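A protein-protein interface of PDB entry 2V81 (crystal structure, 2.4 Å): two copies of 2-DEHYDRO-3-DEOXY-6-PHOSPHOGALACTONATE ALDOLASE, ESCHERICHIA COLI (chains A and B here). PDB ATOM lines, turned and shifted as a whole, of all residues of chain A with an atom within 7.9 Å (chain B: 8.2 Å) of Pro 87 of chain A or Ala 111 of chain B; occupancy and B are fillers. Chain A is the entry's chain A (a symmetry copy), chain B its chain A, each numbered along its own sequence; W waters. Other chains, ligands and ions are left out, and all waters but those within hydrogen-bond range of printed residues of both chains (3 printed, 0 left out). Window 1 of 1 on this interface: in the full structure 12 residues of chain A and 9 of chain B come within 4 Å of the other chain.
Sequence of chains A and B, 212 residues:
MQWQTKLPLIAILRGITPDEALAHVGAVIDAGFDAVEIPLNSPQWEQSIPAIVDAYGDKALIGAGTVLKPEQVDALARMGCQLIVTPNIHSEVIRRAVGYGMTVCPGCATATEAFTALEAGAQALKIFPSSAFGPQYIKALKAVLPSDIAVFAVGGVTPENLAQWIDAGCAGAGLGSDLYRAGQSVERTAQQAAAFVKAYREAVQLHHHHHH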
ATOM      1  N   GLY A  65     -23.974  21.545  -5.153  1.00  0.00           N
ATOM      2  CA  GLY A  65     -23.314  20.747  -6.183  1.00  0.00           C
ATOM      3  C   GLY A  65     -24.268  19.693  -6.687  1.00  0.00           C
ATOM      4  O   GLY A  65     -25.367  19.527  -6.121  1.00  0.00           O
ATOM      5  N   THR A  66     -23.861  18.979  -7.747  1.00  0.00           N
ATOM      6  CA  THR A  66     -24.698  17.950  -8.391  1.00  0.00           C
ATOM      7  C   THR A  66     -26.061  18.506  -8.842  1.00  0.00           C
ATOM      8  O   THR A  66     -27.085  17.816  -8.768  1.00  0.00           O
ATOM      9  CB  THR A  66     -24.888  16.699  -7.465  1.00  0.00           C
ATOM     10  OG1 THR A  66     -23.698  16.494  -6.679  1.00  0.00           O
ATOM     11  CG2 THR A  66     -25.165  15.428  -8.296  1.00  0.00           C
ATOM     12  N   VAL A  67     -26.082  19.758  -9.303  1.00  0.00           N
ATOM     13  CA  VAL A  67     -27.341  20.383  -9.742  1.00  0.00           C
ATOM     14  C   VAL A  67     -27.613  20.008 -11.202  1.00  0.00           C
ATOM     15  O   VAL A  67     -26.877  20.417 -12.099  1.00  0.00           O
ATOM     16  CB  VAL A  67     -27.326  21.917  -9.538  1.00  0.00           C
ATOM     17  CG1 VAL A  67     -28.653  22.551  -9.983  1.00  0.00           C
ATOM     18  CG2 VAL A  67     -27.014  22.268  -8.073  1.00  0.00           C
ATOM     19  N   LEU A  68     -28.662  19.216 -11.421  1.00  0.00           N
ATOM     20  CA  LEU A  68     -28.941  18.608 -12.730  1.00  0.00           C
ATOM     21  C   LEU A  68     -30.181  19.158 -13.459  1.00  0.00           C
ATOM     22  O   LEU A  68     -30.329  18.957 -14.668  1.00  0.00           O
ATOM     23  CB  LEU A  68     -29.070  17.076 -12.592  1.00  0.00           C
ATOM     24  CG  LEU A  68     -27.849  16.274 -12.113  1.00  0.00           C
ATOM     25  CD1 LEU A  68     -28.196  14.802 -11.821  1.00  0.00           C
ATOM     26  CD2 LEU A  68     -26.695  16.375 -13.109  1.00  0.00           C
ATOM     27  N   VAL A  85     -22.639  24.386  -8.634  1.00  0.00           N
ATOM     28  CA  VAL A  85     -21.642  23.491  -9.240  1.00  0.00           C
ATOM     29  C   VAL A  85     -22.350  22.258  -9.852  1.00  0.00           C
ATOM     30  O   VAL A  85     -23.378  21.803  -9.333  1.00  0.00           O
ATOM     31  CB  VAL A  85     -20.511  23.090  -8.224  1.00  0.00           C
ATOM     32  CG1 VAL A  85     -19.486  22.143  -8.867  1.00  0.00           C
ATOM     33  CG2 VAL A  85     -19.801  24.348  -7.636  1.00  0.00           C
ATOM     34  N   THR A  86     -21.807  21.739 -10.960  1.00  0.00           N
ATOM     35  CA  THR A  86     -22.450  20.652 -11.742  1.00  0.00           C
ATOM     36  C   THR A  86     -21.440  19.636 -12.309  1.00  0.00           C
ATOM     37  O   THR A  86     -20.264  19.966 -12.499  1.00  0.00           O
ATOM     38  CB  THR A  86     -23.280  21.207 -12.941  1.00  0.00           C
ATOM     39  OG1 THR A  86     -22.393  21.629 -13.984  1.00  0.00           O
ATOM     40  CG2 THR A  86     -24.195  22.371 -12.521  1.00  0.00           C
ATOM     41  N   PRO A  87     -21.887  18.396 -12.578  1.00  0.00           N
ATOM     42  CA  PRO A  87     -20.985  17.445 -13.240  1.00  0.00           C
ATOM     43  C   PRO A  87     -20.940  17.592 -14.766  1.00  0.00           C
ATOM     44  O   PRO A  87     -19.984  17.119 -15.410  1.00  0.00           O
ATOM     45  CB  PRO A  87     -21.588  16.084 -12.877  1.00  0.00           C
ATOM     46  CG  PRO A  87     -23.038  16.345 -12.714  1.00  0.00           C
ATOM     47  CD  PRO A  87     -23.198  17.787 -12.269  1.00  0.00           C
ATOM     48  N   ASN A  88     -21.959  18.238 -15.326  1.00  0.00           N
ATOM     49  CA  ASN A  88     -22.189  18.256 -16.770  1.00  0.00           C
ATOM     50  C   ASN A  88     -22.574  19.645 -17.259  1.00  0.00           C
ATOM     51  O   ASN A  88     -22.871  20.536 -16.446  1.00  0.00           O
ATOM     52  CB  ASN A  88     -23.304  17.270 -17.118  1.00  0.00           C
ATOM     53  CG  ASN A  88     -24.658  17.691 -16.555  1.00  0.00           C
ATOM     54  OD1 ASN A  88     -24.736  18.418 -15.555  1.00  0.00           O
ATOM     55  ND2 ASN A  88     -25.730  17.232 -17.190  1.00  0.00           N
ATOM     56  N   ILE A  89     -22.580  19.824 -18.580  1.00  0.00           N
ATOM     57  CA  ILE A  89     -23.071  21.061 -19.183  1.00  0.00           C
ATOM     58  C   ILE A  89     -24.532  20.916 -19.589  1.00  0.00           C
ATOM     59  O   ILE A  89     -24.864  20.154 -20.496  1.00  0.00           O
ATOM     60  CB  ILE A  89     -22.204  21.544 -20.408  1.00  0.00           C
ATOM     61  CG1 ILE A  89     -20.731  21.756 -20.017  1.00  0.00           C
ATOM     62  CG2 ILE A  89     -22.805  22.813 -21.061  1.00  0.00           C
ATOM     63  CD1 ILE A  89     -20.500  22.479 -18.670  1.00  0.00           C
ATOM     64  N   HIS A  90     -25.392  21.651 -18.894  1.00  0.00           N
ATOM     65  CA  HIS A  90     -26.811  21.760 -19.228  1.00  0.00           C
ATOM     66  C   HIS A  90     -27.111  23.262 -19.377  1.00  0.00           C
ATOM     67  O   HIS A  90     -27.131  24.008 -18.387  1.00  0.00           O
ATOM     68  CB  HIS A  90     -27.662  21.122 -18.120  1.00  0.00           C
ATOM     69  CG  HIS A  90     -29.124  21.038 -18.441  1.00  0.00           C
ATOM     70  ND1 HIS A  90     -29.804  19.840 -18.494  1.00  0.00           N
ATOM     71  CD2 HIS A  90     -30.035  21.999 -18.724  1.00  0.00           C
ATOM     72  CE1 HIS A  90     -31.071  20.066 -18.794  1.00  0.00           C
ATOM     73  NE2 HIS A  90     -31.237  21.368 -18.940  1.00  0.00           N
ATOM     74  N   CYS A 105     -20.264  27.388 -11.797  1.00  0.00           N
ATOM     75  CA  CYS A 105     -19.032  26.717 -12.201  1.00  0.00           C
ATOM     76  C   CYS A 105     -19.346  25.294 -12.676  1.00  0.00           C
ATOM     77  O   CYS A 105     -19.197  24.330 -11.922  1.00  0.00           O
ATOM     78  CB  CYS A 105     -18.020  26.721 -11.048  1.00  0.00           C
ATOM     79  SG  CYS A 105     -16.419  25.998 -11.458  1.00  0.00           S
ATOM     80  N   PRO A 106     -19.776  25.156 -13.944  1.00  0.00           N
ATOM     81  CA  PRO A 106     -20.265  23.878 -14.434  1.00  0.00           C
ATOM     82  C   PRO A 106     -19.161  22.957 -14.968  1.00  0.00           C
ATOM     83  O   PRO A 106     -18.116  23.430 -15.421  1.00  0.00           O
ATOM     84  CB  PRO A 106     -21.228  24.289 -15.549  1.00  0.00           C
ATOM     85  CG  PRO A 106     -20.682  25.566 -16.069  1.00  0.00           C
ATOM     86  CD  PRO A 106     -19.842  26.198 -14.982  1.00  0.00           C
ATOM     87  N   GLY A 107     -19.417  21.654 -14.917  1.00  0.00           N
ATOM     88  CA  GLY A 107     -18.426  20.644 -15.267  1.00  0.00           C
ATOM     89  C   GLY A 107     -18.416  20.224 -16.727  1.00  0.00           C
ATOM     90  O   GLY A 107     -19.456  19.852 -17.296  1.00  0.00           O
ATOM     91  N   CYS A 108     -17.232  20.271 -17.334  1.00  0.00           N
ATOM     92  CA  CYS A 108     -17.054  19.812 -18.710  1.00  0.00           C
ATOM     93  C   CYS A 108     -15.777  18.989 -18.827  1.00  0.00           C
ATOM     94  O   CYS A 108     -14.955  18.960 -17.900  1.00  0.00           O
ATOM     95  CB  CYS A 108     -17.034  20.997 -19.685  1.00  0.00           C
ATOM     96  SG  CYS A 108     -15.773  22.215 -19.305  1.00  0.00           S
ATOM     97  N   ALA A 109     -15.624  18.323 -19.969  1.00  0.00           N
ATOM     98  CA  ALA A 109     -14.493  17.448 -20.195  1.00  0.00           C
ATOM     99  C   ALA A 109     -13.806  17.740 -21.525  1.00  0.00           C
ATOM    100  O   ALA A 109     -12.672  17.306 -21.744  1.00  0.00           O
ATOM    101  CB  ALA A 109     -14.921  15.966 -20.109  1.00  0.00           C
ATOM    102  N   GLU A 113     -17.700  21.182 -25.165  1.00  0.00           N
ATOM    103  CA  GLU A 113     -18.526  21.382 -23.977  1.00  0.00           C
ATOM    104  C   GLU A 113     -18.191  22.681 -23.218  1.00  0.00           C
ATOM    105  O   GLU A 113     -19.077  23.315 -22.620  1.00  0.00           O
ATOM    106  CB  GLU A 113     -18.399  20.175 -23.041  1.00  0.00           C
ATOM    107  CG  GLU A 113     -18.993  18.878 -23.597  1.00  0.00           C
ATOM    108  CD  GLU A 113     -18.640  17.664 -22.761  1.00  0.00           C
ATOM    109  OE1 GLU A 113     -17.880  17.824 -21.789  1.00  0.00           O
ATOM    110  OE2 GLU A 113     -19.114  16.551 -23.071  1.00  0.00           O
ATOM    111  N   LYS A 126     -15.421  24.146 -14.586  1.00  0.00           N
ATOM    112  CA  LYS A 126     -14.902  22.991 -13.867  1.00  0.00           C
ATOM    113  C   LYS A 126     -14.506  21.911 -14.888  1.00  0.00           C
ATOM    114  O   LYS A 126     -15.318  21.529 -15.731  1.00  0.00           O
ATOM    115  CB  LYS A 126     -15.962  22.489 -12.870  1.00  0.00           C
ATOM    116  CG  LYS A 126     -15.895  21.010 -12.496  1.00  0.00           C
ATOM    117  CD  LYS A 126     -17.050  20.624 -11.578  1.00  0.00           C
ATOM    118  CE  LYS A 126     -17.081  19.121 -11.340  1.00  0.00           C
ATOM    119  NZ  LYS A 126     -18.272  18.676 -10.546  1.00  0.00           N
ATOM    120  N   ILE A 127     -13.249  21.463 -14.833  1.00  0.00           N
ATOM    121  CA  ILE A 127     -12.787  20.353 -15.654  1.00  0.00           C
ATOM    122  C   ILE A 127     -12.846  19.086 -14.797  1.00  0.00           C
ATOM    123  O   ILE A 127     -12.167  18.986 -13.761  1.00  0.00           O
ATOM    124  CB  ILE A 127     -11.350  20.572 -16.239  1.00  0.00           C
ATOM    125  CG1 ILE A 127     -11.178  21.985 -16.835  1.00  0.00           C
ATOM    126  CG2 ILE A 127     -10.992  19.480 -17.272  1.00  0.00           C
ATOM    127  CD1 ILE A 127     -12.073  22.312 -18.045  1.00  0.00           C
ATOM    128  N   PHE A 128     -13.666  18.133 -15.237  1.00  0.00           N
ATOM    129  CA  PHE A 128     -14.020  16.973 -14.427  1.00  0.00           C
ATOM    130  C   PHE A 128     -14.259  15.721 -15.275  1.00  0.00           C
ATOM    131  O   PHE A 128     -15.075  15.751 -16.204  1.00  0.00           O
ATOM    132  CB  PHE A 128     -15.267  17.285 -13.588  1.00  0.00           C
ATOM    133  CG  PHE A 128     -15.847  16.094 -12.879  1.00  0.00           C
ATOM    134  CD1 PHE A 128     -15.257  15.602 -11.709  1.00  0.00           C
ATOM    135  CD2 PHE A 128     -16.999  15.469 -13.374  1.00  0.00           C
ATOM    136  CE1 PHE A 128     -15.790  14.491 -11.043  1.00  0.00           C
ATOM    137  CE2 PHE A 128     -17.551  14.354 -12.719  1.00  0.00           C
ATOM    138  CZ  PHE A 128     -16.942  13.861 -11.549  1.00  0.00           C
ATOM    139  N   PRO A 129     -13.583  14.602 -14.924  1.00  0.00           N
ATOM    140  CA  PRO A 129     -12.650  14.456 -13.801  1.00  0.00           C
ATOM    141  C   PRO A 129     -11.189  14.708 -14.164  1.00  0.00           C
ATOM    142  O   PRO A 129     -10.660  14.078 -15.074  1.00  0.00           O
ATOM    143  CB  PRO A 129     -12.849  13.002 -13.375  1.00  0.00           C
ATOM    144  CG  PRO A 129     -13.330  12.293 -14.612  1.00  0.00           C
ATOM    145  CD  PRO A 129     -13.763  13.324 -15.633  1.00  0.00           C
ATOM    146  N   CYS B 108     -20.583   6.484 -24.573  1.00  0.00           N
ATOM    147  CA  CYS B 108     -20.257   7.868 -24.239  1.00  0.00           C
ATOM    148  C   CYS B 108     -18.854   7.949 -23.651  1.00  0.00           C
ATOM    149  O   CYS B 108     -18.243   6.921 -23.324  1.00  0.00           O
ATOM    150  CB  CYS B 108     -21.292   8.459 -23.271  1.00  0.00           C
ATOM    151  SG  CYS B 108     -21.472   7.517 -21.756  1.00  0.00           S
ATOM    152  N   ALA B 109     -18.352   9.175 -23.523  1.00  0.00           N
ATOM    153  CA  ALA B 109     -17.006   9.401 -23.041  1.00  0.00           C
ATOM    154  C   ALA B 109     -16.971  10.436 -21.920  1.00  0.00           C
ATOM    155  O   ALA B 109     -15.973  10.535 -21.202  1.00  0.00           O
ATOM    156  CB  ALA B 109     -16.070   9.811 -24.200  1.00  0.00           C
ATOM    157  N   THR B 110     -18.044  11.215 -21.780  1.00  0.00           N
ATOM    158  CA  THR B 110     -18.092  12.269 -20.754  1.00  0.00           C
ATOM    159  C   THR B 110     -19.359  12.206 -19.903  1.00  0.00           C
ATOM    160  O   THR B 110     -20.332  11.516 -20.258  1.00  0.00           O
ATOM    161  CB  THR B 110     -17.975  13.699 -21.356  1.00  0.00           C
ATOM    162  OG1 THR B 110     -19.240  14.115 -21.886  1.00  0.00           O
ATOM    163  CG2 THR B 110     -16.896  13.782 -22.441  1.00  0.00           C
ATOM    164  N   ALA B 111     -19.332  12.942 -18.788  1.00  0.00           N
ATOM    165  CA  ALA B 111     -20.485  13.099 -17.895  1.00  0.00           C
ATOM    166  C   ALA B 111     -21.683  13.724 -18.611  1.00  0.00           C
ATOM    167  O   ALA B 111     -22.801  13.243 -18.476  1.00  0.00           O
ATOM    168  CB  ALA B 111     -20.102  13.915 -16.649  1.00  0.00           C
ATOM    169  N   THR B 112     -21.437  14.773 -19.394  1.00  0.00           N
ATOM    170  CA  THR B 112     -22.481  15.422 -20.195  1.00  0.00           C
ATOM    171  C   THR B 112     -23.195  14.427 -21.133  1.00  0.00           C
ATOM    172  O   THR B 112     -24.431  14.322 -21.114  1.00  0.00           O
ATOM    173  CB  THR B 112     -21.904  16.606 -21.003  1.00  0.00           C
ATOM    174  OG1 THR B 112     -21.318  17.557 -20.103  1.00  0.00           O
ATOM    175  CG2 THR B 112     -22.992  17.291 -21.836  1.00  0.00           C
ATOM    176  N   GLU B 113     -22.412  13.697 -21.929  1.00  0.00           N
ATOM    177  CA  GLU B 113     -22.939  12.690 -22.846  1.00  0.00           C
ATOM    178  C   GLU B 113     -23.694  11.554 -22.130  1.00  0.00           C
ATOM    179  O   GLU B 113     -24.663  10.994 -22.671  1.00  0.00           O
ATOM    180  CB  GLU B 113     -21.802  12.113 -23.698  1.00  0.00           C
ATOM    181  CG  GLU B 113     -21.180  13.110 -24.681  1.00  0.00           C
ATOM    182  CD  GLU B 113     -19.915  12.584 -25.329  1.00  0.00           C
ATOM    183  OE1 GLU B 113     -19.488  11.474 -24.964  1.00  0.00           O
ATOM    184  OE2 GLU B 113     -19.342  13.274 -26.198  1.00  0.00           O
ATOM    185  N   ALA B 114     -23.247  11.213 -20.923  1.00  0.00           N
ATOM    186  CA  ALA B 114     -23.871  10.136 -20.168  1.00  0.00           C
ATOM    187  C   ALA B 114     -25.256  10.548 -19.663  1.00  0.00           C
ATOM    188  O   ALA B 114     -26.193   9.768 -19.774  1.00  0.00           O
ATOM    189  CB  ALA B 114     -22.974   9.676 -19.021  1.00  0.00           C
ATOM    190  N   PHE B 115     -25.386  11.769 -19.128  1.00  0.00           N
ATOM    191  CA  PHE B 115     -26.689  12.255 -18.647  1.00  0.00           C
ATOM    192  C   PHE B 115     -27.699  12.442 -19.795  1.00  0.00           C
ATOM    193  O   PHE B 115     -28.888  12.138 -19.643  1.00  0.00           O
ATOM    194  CB  PHE B 115     -26.544  13.518 -17.795  1.00  0.00           C
ATOM    195  CG  PHE B 115     -26.039  13.251 -16.390  1.00  0.00           C
ATOM    196  CD1 PHE B 115     -26.852  12.612 -15.445  1.00  0.00           C
ATOM    197  CD2 PHE B 115     -24.758  13.645 -16.008  1.00  0.00           C
ATOM    198  CE1 PHE B 115     -26.396  12.360 -14.145  1.00  0.00           C
ATOM    199  CE2 PHE B 115     -24.290  13.400 -14.714  1.00  0.00           C
ATOM    200  CZ  PHE B 115     -25.114  12.756 -13.779  1.00  0.00           C
ATOM    201  N   THR B 116     -27.208  12.927 -20.937  1.00  0.00           N
ATOM    202  CA  THR B 116     -27.966  12.941 -22.194  1.00  0.00           C
ATOM    203  C   THR B 116     -28.527  11.547 -22.558  1.00  0.00           C
ATOM    204  O   THR B 116     -29.707  11.419 -22.906  1.00  0.00           O
ATOM    205  CB  THR B 116     -27.101  13.496 -23.358  1.00  0.00           C
ATOM    206  OG1 THR B 116     -26.605  14.794 -22.999  1.00  0.00           O
ATOM    207  CG2 THR B 116     -27.902  13.621 -24.637  1.00  0.00           C
ATOM    208  N   ALA B 117     -27.697  10.513 -22.447  1.00  0.00           N
ATOM    209  CA  ALA B 117     -28.098   9.151 -22.831  1.00  0.00           C
ATOM    210  C   ALA B 117     -29.210   8.603 -21.936  1.00  0.00           C
ATOM    211  O   ALA B 117     -30.104   7.891 -22.401  1.00  0.00           O
ATOM    212  CB  ALA B 117     -26.899   8.210 -22.837  1.00  0.00           C
ATOM    213  N   LEU B 118     -29.140   8.950 -20.653  1.00  0.00           N
ATOM    214  CA  LEU B 118     -30.128   8.528 -19.668  1.00  0.00           C
ATOM    215  C   LEU B 118     -31.485   9.198 -19.871  1.00  0.00           C
ATOM    216  O   LEU B 118     -32.521   8.577 -19.634  1.00  0.00           O
ATOM    217  CB  LEU B 118     -29.610   8.800 -18.249  1.00  0.00           C
ATOM    218  CG  LEU B 118     -28.346   8.043 -17.831  1.00  0.00           C
ATOM    219  CD1 LEU B 118     -27.841   8.558 -16.489  1.00  0.00           C
ATOM    220  CD2 LEU B 118     -28.588   6.539 -17.784  1.00  0.00           C
ATOM    221  N   LEU B 125     -25.082   1.920 -19.781  1.00  0.00           N
ATOM    222  CA  LEU B 125     -24.131   2.830 -20.430  1.00  0.00           C
ATOM    223  C   LEU B 125     -22.828   2.132 -20.786  1.00  0.00           C
ATOM    224  O   LEU B 125     -22.316   1.312 -20.014  1.00  0.00           O
ATOM    225  CB  LEU B 125     -23.825   4.065 -19.567  1.00  0.00           C
ATOM    226  CG  LEU B 125     -24.950   5.060 -19.265  1.00  0.00           C
ATOM    227  CD1 LEU B 125     -24.445   6.192 -18.360  1.00  0.00           C
ATOM    228  CD2 LEU B 125     -25.580   5.613 -20.544  1.00  0.00           C
ATOM    229  N   ILE B 127     -18.901   3.010 -21.633  1.00  0.00           N
ATOM    230  CA  ILE B 127     -17.828   3.994 -21.607  1.00  0.00           C
ATOM    231  C   ILE B 127     -16.763   3.546 -22.611  1.00  0.00           C
ATOM    232  O   ILE B 127     -16.170   2.463 -22.470  1.00  0.00           O
ATOM    233  CB  ILE B 127     -17.209   4.198 -20.181  1.00  0.00           C
ATOM    234  CG1 ILE B 127     -18.296   4.339 -19.096  1.00  0.00           C
ATOM    235  CG2 ILE B 127     -16.235   5.397 -20.159  1.00  0.00           C
ATOM    236  CD1 ILE B 127     -19.216   5.566 -19.227  1.00  0.00           C
ATOM    237  N   TYR B 137     -11.129   7.004 -14.029  1.00  0.00           N
ATOM    238  CA  TYR B 137     -12.114   7.788 -14.789  1.00  0.00           C
ATOM    239  C   TYR B 137     -13.527   7.245 -14.567  1.00  0.00           C
ATOM    240  O   TYR B 137     -14.448   8.001 -14.242  1.00  0.00           O
ATOM    241  CB  TYR B 137     -11.773   7.779 -16.284  1.00  0.00           C
ATOM    242  CG  TYR B 137     -12.541   8.794 -17.114  1.00  0.00           C
ATOM    243  CD1 TYR B 137     -12.078  10.104 -17.250  1.00  0.00           C
ATOM    244  CD2 TYR B 137     -13.719   8.442 -17.772  1.00  0.00           C
ATOM    245  CE1 TYR B 137     -12.776  11.041 -18.018  1.00  0.00           C
ATOM    246  CE2 TYR B 137     -14.424   9.371 -18.536  1.00  0.00           C
ATOM    247  CZ  TYR B 137     -13.949  10.670 -18.652  1.00  0.00           C
ATOM    248  OH  TYR B 137     -14.637  11.593 -19.404  1.00  0.00           O
ATOM    249  N   ALA B 140     -14.804   7.794 -11.019  1.00  0.00           N
ATOM    250  CA  ALA B 140     -15.146   9.210 -10.836  1.00  0.00           C
ATOM    251  C   ALA B 140     -16.546   9.521 -11.364  1.00  0.00           C
ATOM    252  O   ALA B 140     -17.293  10.274 -10.739  1.00  0.00           O
ATOM    253  CB  ALA B 140     -14.104  10.109 -11.492  1.00  0.00           C
ATOM    254  N   LEU B 141     -16.895   8.922 -12.504  1.00  0.00           N
ATOM    255  CA  LEU B 141     -18.230   9.059 -13.092  1.00  0.00           C
ATOM    256  C   LEU B 141     -19.303   8.408 -12.228  1.00  0.00           C
ATOM    257  O   LEU B 141     -20.300   9.052 -11.881  1.00  0.00           O
ATOM    258  CB  LEU B 141     -18.268   8.477 -14.512  1.00  0.00           C
ATOM    259  CG  LEU B 141     -17.528   9.231 -15.625  1.00  0.00           C
ATOM    260  CD1 LEU B 141     -17.720   8.530 -16.974  1.00  0.00           C
ATOM    261  CD2 LEU B 141     -17.969  10.692 -15.707  1.00  0.00           C
ATOM    262  N   ALA B 143     -19.512   7.956  -9.245  1.00  0.00           N
ATOM    263  CA  ALA B 143     -19.752   8.717  -8.030  1.00  0.00           C
ATOM    264  C   ALA B 143     -20.770   9.837  -8.235  1.00  0.00           C
ATOM    265  O   ALA B 143     -21.219  10.460  -7.273  1.00  0.00           O
ATOM    266  CB  ALA B 143     -18.440   9.282  -7.502  1.00  0.00           C
ATOM    267  N   VAL B 144     -21.132  10.089  -9.489  1.00  0.00           N
ATOM    268  CA  VAL B 144     -22.018  11.207  -9.812  1.00  0.00           C
ATOM    269  C   VAL B 144     -23.261  10.767 -10.613  1.00  0.00           C
ATOM    270  O   VAL B 144     -24.288  11.451 -10.609  1.00  0.00           O
ATOM    271  CB  VAL B 144     -21.231  12.377 -10.487  1.00  0.00           C
ATOM    272  CG1 VAL B 144     -20.998  12.111 -12.006  1.00  0.00           C
ATOM    273  CG2 VAL B 144     -21.949  13.703 -10.248  1.00  0.00           C
ATOM    274  N   LEU B 145     -23.155   9.620 -11.279  1.00  0.00           N
ATOM    275  CA  LEU B 145     -24.296   8.988 -11.930  1.00  0.00           C
ATOM    276  C   LEU B 145     -25.226   8.341 -10.881  1.00  0.00           C
ATOM    277  O   LEU B 145     -24.794   8.072  -9.753  1.00  0.00           O
ATOM    278  CB  LEU B 145     -23.807   7.943 -12.939  1.00  0.00           C
ATOM    279  CG  LEU B 145     -22.885   8.400 -14.079  1.00  0.00           C
ATOM    280  CD1 LEU B 145     -22.265   7.196 -14.779  1.00  0.00           C
ATOM    281  CD2 LEU B 145     -23.628   9.279 -15.081  1.00  0.00           C
HETATM  282  O   HOH W   1     -18.927  16.341 -19.487  1.00  0.00           O
HETATM  283  O   HOH W   2     -16.480  13.468 -17.895  1.00  0.00           O
HETATM  284  O   HOH W   3     -25.819  16.330 -19.810  1.00  0.00           O
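OE2 of Glu 113 of chain A sits at hydrogen-bond distance from OG1 of Thr 110 of chain B (2.7 Å). OG1 of Thr 112 of chain B lies within hydrogen-bond range of N of Ile 89 of chain A, at 3.0 Å.
Water W1 lies within hydrogen-bond range of the side-chain hydroxyl (OG1) of Thr 112 of chain B (2.8 Å), the side-chain carboxylate (OE1) of Glu 113 of chain A (2.9 Å), the side-chain hydroxyl (OG1) of Thr 110 of chain B (3.3 Å) and the backbone NH (N) of Ala 111 of chain B (3.5 Å). Water W3 lies within hydrogen-bond range of O of Thr 112 of chain B (2.8 Å) and ND2 of Asn 88 of chain A (2.8 Å). Water W2 lies within hydrogen-bond range of the side-chain hydroxyl of Tyr 137 of chain B (3.0 Å), the backbone NH of Ala 111 of chain B (3.0 Å) and the backbone carbonyl oxygen of Phe 128 of chain A (3.2 Å).
Pro 87 of chain A touches three residues of chain B. Ala 111 of chain B touches just one residue of chain A: Pro 87 (3.4 Å). Printed residues of chain B within 4 Å of Phe 128 of chain A: Ala 140 (3.7 Å). Of the printed residues of chain A, Thr 112 of chain B touches Asn 88 (3.5 Å), Ile 89 (3.0 Å) and Glu 113 (3.5 Å). Of the printed residues of chain B, Ile 89 of chain A touches Thr 112 (3.0 Å). The nearest residue of chain B that does not touch Pro 87 of chain A is Thr 112 of chain B (4.8 Å). The nearest residue of chain A that does not touch Ala 111 of chain B is Asn 88 of chain A (4.2 Å).
Positions printed for both chains: 108, 109, 113 and 127. Of the 13 pairs that touch across the chains among the printed residues, none has its exchanged pair printed and touching as well.
Of the 20 printed residues of chain A, 8 touch a printed residue of chain B. Printed residues of chain A that touch a printed residue of chain B: Leu 68, Pro 87, Asn 88, Ile 89, Ala 109, Glu 113, Phe 128 and Pro 129. Hydrophobic or aromatic side chains of chain A within 4 Å of the printed part of chain B: Leu 68, Pro 87, Ala 109, Phe 128 and Pro 129. Printed residues of chain B that touch a printed residue of chain A: Thr 110, Ala 111, Thr 112, Phe 115, Tyr 137, Ala 140 and Val 144. Among the printed residues, 13 pairs touch across the chains.
N of Ala 109 of chain A lies within hydrogen-bond range of OE1 of Glu 113 of chain A (2.9 Å). O of Asn 88 of chain A sits at hydrogen-bond distance from OG1 of Thr 86 of chain A. The backbone carbonyl oxygen (O) of Ala 109 of chain B lies within hydrogen-bond range of the side-chain hydroxyl (OH) of Tyr 137 of chain B (2.5 Å). The backbone carbonyl oxygen (O) of Cys 108 of chain A sits at hydrogen-bond distance from the backbone NH (N) of Phe 128 of chain A. N of Thr 112 of chain B sits close to OG1 of Thr 110 of chain B. The backbone NH (N) of Glu 113 of chain B sits at hydrogen-bond distance from the side-chain hydroxyl (OG1) of Thr 110 of chain B (3.2 Å).
Among the printed residues, merely in contact across the chains: Pro 87 of chain A with Ala 111 of chain B, Pro 129 of chain A with Tyr 137 of chain B, Glu 113 of chain A with Thr 112 of chain B, Asn 88 of chain A with Thr 112 of chain B, Pro 87 of chain A with Val 144 of chain B, Pro 129 of chain A with Ala 140 of chain B, Phe 128 of chain A with Ala 140 of chain B, Ala 109 of chain A with Thr 110 of chain B, Pro 87 of chain A with Phe 115 of chain B, Leu 68 of chain A with Phe 115 of chain B and Asn 88 of chain A with Phe 115 of chain B.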
